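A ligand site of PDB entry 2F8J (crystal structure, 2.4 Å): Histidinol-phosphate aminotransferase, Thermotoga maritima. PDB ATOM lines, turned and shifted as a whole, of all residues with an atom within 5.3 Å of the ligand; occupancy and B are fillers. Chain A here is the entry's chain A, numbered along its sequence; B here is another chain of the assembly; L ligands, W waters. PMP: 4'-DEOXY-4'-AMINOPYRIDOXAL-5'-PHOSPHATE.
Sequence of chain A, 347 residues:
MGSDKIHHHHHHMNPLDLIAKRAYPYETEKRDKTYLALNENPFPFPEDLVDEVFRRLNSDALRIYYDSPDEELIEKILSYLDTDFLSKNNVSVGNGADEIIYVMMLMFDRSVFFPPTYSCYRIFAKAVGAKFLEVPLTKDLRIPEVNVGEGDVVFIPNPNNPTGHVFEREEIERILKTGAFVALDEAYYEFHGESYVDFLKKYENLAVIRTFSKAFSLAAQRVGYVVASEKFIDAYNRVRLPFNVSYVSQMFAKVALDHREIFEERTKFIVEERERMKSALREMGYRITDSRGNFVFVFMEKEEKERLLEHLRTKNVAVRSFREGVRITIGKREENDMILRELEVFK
Water W1 lies within hydrogen-bond range of the side-chain carboxylate of Asp 98 (2.8 Å), a nitrogen (N4A) of the ligand (3.1 Å) and the side-chain hydroxyl of Tyr 118 (3.4 Å).
OH of Tyr 118 lies within hydrogen-bond range of N4A of the ligand.
An oxygen (O1P) of the ligand is in hydrogen-bond range of the side-chain hydroxyl of Thr 211 (2.6 Å).
OD2 of Asp 185 sits at hydrogen-bond distance from N1 of the ligand.
An oxygen (O3P) of the ligand is in salt-bridge range of the guanidinium group of Arg 222, at 2.7 Å.
The side-chain amide nitrogen (ND2) of Asn 161 sits at hydrogen-bond distance from an oxygen (O3) of the ligand.
OH of Tyr 65 of chain B sits at hydrogen-bond distance from O2P of the ligand (2.8 Å).
OH of Tyr 188 lies within hydrogen-bond range of O3 of the ligand, 2.9 Å away.
An oxygen (O2P) of the ligand is in hydrogen-bond range of the side-chain hydroxyl (OG) of Ser 213.
An oxygen (O1P) of the ligand lies within hydrogen-bond range of the backbone NH of Ala 97 (2.9 Å).
N of Asp 98 lies within hydrogen-bond range of O3P of the ligand.
Residues that only touch the ligand: Lys 214, Gly 96, Ala 187 and Ile 101.
Hydrophobic or aromatic side chains that line the ligand: Ala 97, Ile 101, Tyr 118, Ala 187, Tyr 188 and Tyr 65 of chain B.
Of the 23 residues printed, 14 come within 4 Å of the ligand.
The backbone NH (N) of Ser 213 lies within hydrogen-bond range of the side-chain hydroxyl (OG1) of Thr 211 (3.0 Å).
The backbone carbonyl oxygen (O) of Val 223 lies within hydrogen-bond range of the side-chain hydroxyl (OG1) of Thr 211 (3.5 Å).
The backbone NH (N) of Ala 187 lies close to the side-chain carboxylate (OD1) of Asp 185 (3.4 Å).
The side-chain carboxylate (OD2) of Asp 185 is in hydrogen-bond range of the side-chain hydroxyl (OH) of Tyr 121 (2.7 Å).
The side-chain hydroxyl (OG) of Ser 213 is in hydrogen-bond range of the guanidinium group (NH1) of Arg 222, at 3.5 Å.
The backbone carbonyl oxygen (O) of Arg 222 is in hydrogen-bond range of the backbone NH (N) of Gly 96.
NH1 of Arg 222 sits at hydrogen-bond distance from O of Ala 219 (3.0 Å).
The side-chain hydroxyl (OH) of Tyr 188 lies within hydrogen-bond range of the side-chain amide nitrogen (ND2) of Asn 39 (2.8 Å).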
ATOM      1  N   ASN A  39      27.628   6.893 -10.165  1.00  0.00           N
ATOM      2  CA  ASN A  39      28.407   5.680 -10.098  1.00  0.00           C
ATOM      3  C   ASN A  39      28.770   5.090 -11.472  1.00  0.00           C
ATOM      4  O   ASN A  39      28.909   3.870 -11.619  1.00  0.00           O
ATOM      5  CB  ASN A  39      27.683   4.697  -9.159  1.00  0.00           C
ATOM      6  CG  ASN A  39      27.786   5.149  -7.705  1.00  0.00           C
ATOM      7  OD1 ASN A  39      28.617   5.993  -7.355  1.00  0.00           O
ATOM      8  ND2 ASN A  39      26.947   4.571  -6.851  1.00  0.00           N
ATOM      9  N   ASN A  95      16.233  -4.874 -19.072  1.00  0.00           N
ATOM     10  CA  ASN A  95      16.580  -3.579 -19.626  1.00  0.00           C
ATOM     11  C   ASN A  95      17.156  -2.721 -18.492  1.00  0.00           C
ATOM     12  O   ASN A  95      16.476  -1.903 -17.895  1.00  0.00           O
ATOM     13  CB  ASN A  95      15.334  -2.913 -20.261  1.00  0.00           C
ATOM     14  CG  ASN A  95      15.679  -1.638 -20.969  1.00  0.00           C
ATOM     15  OD1 ASN A  95      16.776  -1.492 -21.456  1.00  0.00           O
ATOM     16  ND2 ASN A  95      14.726  -0.700 -21.044  1.00  0.00           N
ATOM     17  N   GLY A  96      18.424  -2.982 -18.182  1.00  0.00           N
ATOM     18  CA  GLY A  96      19.035  -2.522 -16.953  1.00  0.00           C
ATOM     19  C   GLY A  96      18.649  -3.436 -15.786  1.00  0.00           C
ATOM     20  O   GLY A  96      17.657  -4.145 -15.838  1.00  0.00           O
ATOM     21  N   ALA A  97      19.456  -3.412 -14.739  1.00  0.00           N
ATOM     22  CA  ALA A  97      19.061  -3.973 -13.452  1.00  0.00           C
ATOM     23  C   ALA A  97      17.803  -3.302 -12.920  1.00  0.00           C
ATOM     24  O   ALA A  97      17.014  -3.914 -12.197  1.00  0.00           O
ATOM     25  CB  ALA A  97      20.178  -3.867 -12.476  1.00  0.00           C
ATOM     26  N   ASP A  98      17.618  -2.041 -13.289  1.00  0.00           N
ATOM     27  CA  ASP A  98      16.427  -1.280 -12.928  1.00  0.00           C
ATOM     28  C   ASP A  98      15.141  -2.007 -13.331  1.00  0.00           C
ATOM     29  O   ASP A  98      14.206  -2.044 -12.529  1.00  0.00           O
ATOM     30  CB  ASP A  98      16.458   0.111 -13.574  1.00  0.00           C
ATOM     31  CG  ASP A  98      17.192   1.183 -12.711  1.00  0.00           C
ATOM     32  OD1 ASP A  98      17.755   0.852 -11.651  1.00  0.00           O
ATOM     33  OD2 ASP A  98      17.179   2.372 -13.120  1.00  0.00           O
ATOM     34  N   GLU A  99      15.096  -2.571 -14.551  1.00  0.00           N
ATOM     35  CA  GLU A  99      13.910  -3.304 -14.987  1.00  0.00           C
ATOM     36  C   GLU A  99      13.674  -4.552 -14.148  1.00  0.00           C
ATOM     37  O   GLU A  99      12.536  -4.941 -13.915  1.00  0.00           O
ATOM     38  CB  GLU A  99      13.996  -3.714 -16.460  1.00  0.00           C
ATOM     39  CG  GLU A  99      12.671  -4.258 -17.011  1.00  0.00           C
ATOM     40  CD  GLU A  99      12.760  -4.901 -18.398  1.00  0.00           C
ATOM     41  OE1 GLU A  99      13.692  -5.707 -18.650  1.00  0.00           O
ATOM     42  OE2 GLU A  99      11.875  -4.627 -19.241  1.00  0.00           O
ATOM     43  N   ILE A 101      14.497  -5.093 -10.934  1.00  0.00           N
ATOM     44  CA  ILE A 101      13.912  -4.570  -9.690  1.00  0.00           C
ATOM     45  C   ILE A 101      12.435  -4.213  -9.873  1.00  0.00           C
ATOM     46  O   ILE A 101      11.586  -4.580  -9.046  1.00  0.00           O
ATOM     47  CB  ILE A 101      14.672  -3.287  -9.243  1.00  0.00           C
ATOM     48  CG1 ILE A 101      16.074  -3.665  -8.729  1.00  0.00           C
ATOM     49  CG2 ILE A 101      13.905  -2.516  -8.184  1.00  0.00           C
ATOM     50  CD1 ILE A 101      17.112  -2.628  -9.002  1.00  0.00           C
ATOM     51  N   TYR A 118      19.423   2.011  -2.201  1.00  0.00           N
ATOM     52  CA  TYR A 118      19.243   2.493  -3.556  1.00  0.00           C
ATOM     53  C   TYR A 118      17.989   3.360  -3.672  1.00  0.00           C
ATOM     54  O   TYR A 118      16.902   2.964  -3.254  1.00  0.00           O
ATOM     55  CB  TYR A 118      19.152   1.326  -4.520  1.00  0.00           C
ATOM     56  CG  TYR A 118      19.181   1.718  -5.971  1.00  0.00           C
ATOM     57  CD1 TYR A 118      19.935   2.790  -6.428  1.00  0.00           C
ATOM     58  CD2 TYR A 118      18.503   0.970  -6.908  1.00  0.00           C
ATOM     59  CE1 TYR A 118      19.984   3.114  -7.747  1.00  0.00           C
ATOM     60  CE2 TYR A 118      18.546   1.282  -8.239  1.00  0.00           C
ATOM     61  CZ  TYR A 118      19.286   2.366  -8.662  1.00  0.00           C
ATOM     62  OH  TYR A 118      19.318   2.674 -10.001  1.00  0.00           O
ATOM     63  N   TYR A 121      14.414   2.174  -5.347  1.00  0.00           N
ATOM     64  CA  TYR A 121      13.495   1.224  -4.736  1.00  0.00           C
ATOM     65  C   TYR A 121      12.220   1.933  -4.349  1.00  0.00           C
ATOM     66  O   TYR A 121      11.140   1.505  -4.736  1.00  0.00           O
ATOM     67  CB  TYR A 121      14.111   0.538  -3.518  1.00  0.00           C
ATOM     68  CG  TYR A 121      15.318  -0.341  -3.792  1.00  0.00           C
ATOM     69  CD1 TYR A 121      15.511  -0.926  -5.054  1.00  0.00           C
ATOM     70  CD2 TYR A 121      16.228  -0.621  -2.780  1.00  0.00           C
ATOM     71  CE1 TYR A 121      16.612  -1.735  -5.298  1.00  0.00           C
ATOM     72  CE2 TYR A 121      17.331  -1.455  -3.007  1.00  0.00           C
ATOM     73  CZ  TYR A 121      17.519  -2.006  -4.275  1.00  0.00           C
ATOM     74  OH  TYR A 121      18.611  -2.820  -4.518  1.00  0.00           O
ATOM     75  N   PRO A 157      21.075  -4.404  -1.498  1.00  0.00           N
ATOM     76  CA  PRO A 157      22.271  -4.215  -2.316  1.00  0.00           C
ATOM     77  C   PRO A 157      23.527  -4.643  -1.556  1.00  0.00           C
ATOM     78  O   PRO A 157      23.647  -4.371  -0.377  1.00  0.00           O
ATOM     79  CB  PRO A 157      22.270  -2.719  -2.613  1.00  0.00           C
ATOM     80  CG  PRO A 157      20.976  -2.191  -2.112  1.00  0.00           C
ATOM     81  CD  PRO A 157      20.521  -3.117  -1.059  1.00  0.00           C
ATOM     82  N   ASN A 161      24.420   0.514  -1.576  1.00  0.00           N
ATOM     83  CA  ASN A 161      24.434   1.827  -2.198  1.00  0.00           C
ATOM     84  C   ASN A 161      23.545   2.669  -1.298  1.00  0.00           C
ATOM     85  O   ASN A 161      22.408   2.279  -1.055  1.00  0.00           O
ATOM     86  CB  ASN A 161      23.823   1.726  -3.591  1.00  0.00           C
ATOM     87  CG  ASN A 161      23.978   3.005  -4.438  1.00  0.00           C
ATOM     88  OD1 ASN A 161      24.463   4.044  -3.992  1.00  0.00           O
ATOM     89  ND2 ASN A 161      23.556   2.899  -5.693  1.00  0.00           N
ATOM     90  N   ASP A 185      21.103  -7.418  -4.740  1.00  0.00           N
ATOM     91  CA  ASP A 185      21.468  -6.517  -5.815  1.00  0.00           C
ATOM     92  C   ASP A 185      22.987  -6.348  -5.835  1.00  0.00           C
ATOM     93  O   ASP A 185      23.543  -5.575  -5.052  1.00  0.00           O
ATOM     94  CB  ASP A 185      20.743  -5.183  -5.593  1.00  0.00           C
ATOM     95  CG  ASP A 185      20.825  -4.257  -6.781  1.00  0.00           C
ATOM     96  OD1 ASP A 185      21.697  -4.479  -7.664  1.00  0.00           O
ATOM     97  OD2 ASP A 185      20.009  -3.298  -6.821  1.00  0.00           O
ATOM     98  N   ALA A 187      25.040  -5.028  -8.008  1.00  0.00           N
ATOM     99  CA  ALA A 187      25.443  -4.025  -8.996  1.00  0.00           C
ATOM    100  C   ALA A 187      26.919  -3.647  -8.917  1.00  0.00           C
ATOM    101  O   ALA A 187      27.503  -3.266  -9.943  1.00  0.00           O
ATOM    102  CB  ALA A 187      24.583  -2.765  -8.825  1.00  0.00           C
ATOM    103  N   TYR A 188      27.509  -3.724  -7.712  1.00  0.00           N
ATOM    104  CA  TYR A 188      28.911  -3.328  -7.470  1.00  0.00           C
ATOM    105  C   TYR A 188      29.812  -4.502  -7.170  1.00  0.00           C
ATOM    106  O   TYR A 188      30.942  -4.317  -6.714  1.00  0.00           O
ATOM    107  CB  TYR A 188      28.980  -2.275  -6.333  1.00  0.00           C
ATOM    108  CG  TYR A 188      28.142  -1.054  -6.676  1.00  0.00           C
ATOM    109  CD1 TYR A 188      28.599  -0.136  -7.609  1.00  0.00           C
ATOM    110  CD2 TYR A 188      26.877  -0.873  -6.144  1.00  0.00           C
ATOM    111  CE1 TYR A 188      27.832   0.952  -7.965  1.00  0.00           C
ATOM    112  CE2 TYR A 188      26.097   0.220  -6.498  1.00  0.00           C
ATOM    113  CZ  TYR A 188      26.581   1.127  -7.425  1.00  0.00           C
ATOM    114  OH  TYR A 188      25.844   2.214  -7.825  1.00  0.00           O
ATOM    115  N   THR A 211      24.691  -6.272 -13.376  1.00  0.00           N
ATOM    116  CA  THR A 211      24.621  -5.310 -14.461  1.00  0.00           C
ATOM    117  C   THR A 211      25.938  -5.180 -15.200  1.00  0.00           C
ATOM    118  O   THR A 211      27.009  -5.456 -14.653  1.00  0.00           O
ATOM    119  CB  THR A 211      24.161  -3.904 -13.950  1.00  0.00           C
ATOM    120  OG1 THR A 211      24.056  -2.989 -15.036  1.00  0.00           O
ATOM    121  CG2 THR A 211      25.107  -3.318 -12.922  1.00  0.00           C
ATOM    122  N   PHE A 212      25.831  -4.747 -16.458  1.00  0.00           N
ATOM    123  CA  PHE A 212      26.983  -4.367 -17.281  1.00  0.00           C
ATOM    124  C   PHE A 212      27.303  -2.857 -17.191  1.00  0.00           C
ATOM    125  O   PHE A 212      28.291  -2.390 -17.771  1.00  0.00           O
ATOM    126  CB  PHE A 212      26.702  -4.697 -18.750  1.00  0.00           C
ATOM    127  CG  PHE A 212      26.804  -6.152 -19.049  1.00  0.00           C
ATOM    128  CD1 PHE A 212      25.731  -6.997 -18.823  1.00  0.00           C
ATOM    129  CD2 PHE A 212      27.989  -6.682 -19.558  1.00  0.00           C
ATOM    130  CE1 PHE A 212      25.817  -8.342 -19.098  1.00  0.00           C
ATOM    131  CE2 PHE A 212      28.101  -8.060 -19.829  1.00  0.00           C
ATOM    132  CZ  PHE A 212      27.008  -8.883 -19.588  1.00  0.00           C
ATOM    133  N   SER A 213      26.476  -2.111 -16.481  1.00  0.00           N
ATOM    134  CA  SER A 213      26.525  -0.661 -16.556  1.00  0.00           C
ATOM    135  C   SER A 213      27.770  -0.023 -15.914  1.00  0.00           C
ATOM    136  O   SER A 213      28.281   0.964 -16.441  1.00  0.00           O
ATOM    137  CB  SER A 213      25.250  -0.064 -15.958  1.00  0.00           C
ATOM    138  OG  SER A 213      24.121  -0.403 -16.755  1.00  0.00           O
ATOM    139  N   LYS A 214      28.246  -0.590 -14.797  1.00  0.00           N
ATOM    140  CA  LYS A 214      29.292   0.054 -13.988  1.00  0.00           C
ATOM    141  C   LYS A 214      30.686  -0.388 -14.402  1.00  0.00           C
ATOM    142  O   LYS A 214      31.570   0.439 -14.617  1.00  0.00           O
ATOM    143  CB  LYS A 214      29.106  -0.228 -12.485  1.00  0.00           C
ATOM    144  CG  LYS A 214      27.698  -0.017 -11.912  1.00  0.00           C
ATOM    145  CD  LYS A 214      27.116   1.313 -12.296  1.00  0.00           C
ATOM    146  CE  LYS A 214      26.086   1.785 -11.276  1.00  0.00           C
ATOM    147  NZ  LYS A 214      25.213   0.625 -10.884  1.00  0.00           N
ATOM    148  N   ALA A 219      26.439   1.672 -19.449  1.00  0.00           N
ATOM    149  CA  ALA A 219      25.255   2.270 -18.812  1.00  0.00           C
ATOM    150  C   ALA A 219      24.194   2.782 -19.831  1.00  0.00           C
ATOM    151  O   ALA A 219      22.992   2.705 -19.577  1.00  0.00           O
ATOM    152  CB  ALA A 219      25.679   3.380 -17.875  1.00  0.00           C
ATOM    153  N   ARG A 222      22.027  -0.477 -21.234  1.00  0.00           N
ATOM    154  CA  ARG A 222      21.007  -1.068 -20.379  1.00  0.00           C
ATOM    155  C   ARG A 222      20.942  -2.601 -20.452  1.00  0.00           C
ATOM    156  O   ARG A 222      19.981  -3.166 -20.970  1.00  0.00           O
ATOM    157  CB  ARG A 222      19.590  -0.535 -20.733  1.00  0.00           C
ATOM    158  CG  ARG A 222      19.446   0.929 -21.218  1.00  0.00           C
ATOM    159  CD  ARG A 222      19.915   1.927 -20.218  1.00  0.00           C
ATOM    160  NE  ARG A 222      19.260   1.746 -18.919  1.00  0.00           N
ATOM    161  CZ  ARG A 222      19.870   1.393 -17.796  1.00  0.00           C
ATOM    162  NH1 ARG A 222      21.177   1.164 -17.781  1.00  0.00           N
ATOM    163  NH2 ARG A 222      19.143   1.266 -16.685  1.00  0.00           N
ATOM    164  N   VAL A 223      21.946  -3.290 -19.932  1.00  0.00           N
ATOM    165  CA  VAL A 223      21.877  -4.734 -19.813  1.00  0.00           C
ATOM    166  C   VAL A 223      22.103  -5.155 -18.366  1.00  0.00           C
ATOM    167  O   VAL A 223      23.162  -4.942 -17.797  1.00  0.00           O
ATOM    168  CB  VAL A 223      22.868  -5.463 -20.724  1.00  0.00           C
ATOM    169  CG1 VAL A 223      22.589  -6.972 -20.707  1.00  0.00           C
ATOM    170  CG2 VAL A 223      22.747  -4.954 -22.144  1.00  0.00           C
ATOM    171  N   GLY A 224      21.072  -5.743 -17.773  1.00  0.00           N
ATOM    172  CA  GLY A 224      21.180  -6.339 -16.461  1.00  0.00           C
ATOM    173  C   GLY A 224      20.890  -7.810 -16.642  1.00  0.00           C
ATOM    174  O   GLY A 224      20.343  -8.207 -17.670  1.00  0.00           O
ATOM    175  N   TYR B  65      24.405   7.080 -18.194  1.00  0.00           N
ATOM    176  CA  TYR B  65      22.956   7.010 -18.254  1.00  0.00           C
ATOM    177  C   TYR B  65      22.441   8.080 -19.170  1.00  0.00           C
ATOM    178  O   TYR B  65      22.450   9.271 -18.852  1.00  0.00           O
ATOM    179  CB  TYR B  65      22.344   7.110 -16.859  1.00  0.00           C
ATOM    180  CG  TYR B  65      22.701   5.915 -16.018  1.00  0.00           C
ATOM    181  CD1 TYR B  65      22.047   4.713 -16.195  1.00  0.00           C
ATOM    182  CD2 TYR B  65      23.736   5.973 -15.107  1.00  0.00           C
ATOM    183  CE1 TYR B  65      22.390   3.604 -15.444  1.00  0.00           C
ATOM    184  CE2 TYR B  65      24.090   4.868 -14.347  1.00  0.00           C
ATOM    185  CZ  TYR B  65      23.404   3.685 -14.528  1.00  0.00           C
ATOM    186  OH  TYR B  65      23.767   2.584 -13.769  1.00  0.00           O
HETATM  187  N1  PMP L   1      21.008  -1.445  -8.481  1.00  0.00           N
HETATM  188  C2  PMP L   1      21.784  -0.511  -7.881  1.00  0.00           C
HETATM  189  C2A PMP L   1      22.096  -0.628  -6.372  1.00  0.00           C
HETATM  190  C3  PMP L   1      22.309   0.554  -8.644  1.00  0.00           C
HETATM  191  O3  PMP L   1      23.083   1.494  -8.023  1.00  0.00           O
HETATM  192  C4  PMP L   1      22.022   0.637 -10.018  1.00  0.00           C
HETATM  193  C4A PMP L   1      22.531   1.785 -10.923  1.00  0.00           C
HETATM  194  N4A PMP L   1      21.464   2.714 -11.390  1.00  0.00           N
HETATM  195  C5  PMP L   1      21.208  -0.376 -10.572  1.00  0.00           C
HETATM  196  C6  PMP L   1      20.717  -1.410  -9.769  1.00  0.00           C
HETATM  197  C5A PMP L   1      20.834  -0.358 -12.053  1.00  0.00           C
HETATM  198  O4P PMP L   1      21.799  -0.668 -12.956  1.00  0.00           O
HETATM  199  P   PMP L   1      21.247  -0.511 -14.482  1.00  0.00           P
HETATM  200  O1P PMP L   1      21.771  -1.753 -15.348  1.00  0.00           O
HETATM  201  O2P PMP L   1      22.143   0.700 -14.992  1.00  0.00           O
HETATM  202  O3P PMP L   1      19.786  -0.301 -14.601  1.00  0.00           O
HETATM  203  O   HOH W   1      19.324   4.241 -12.967  1.00  0.00           O
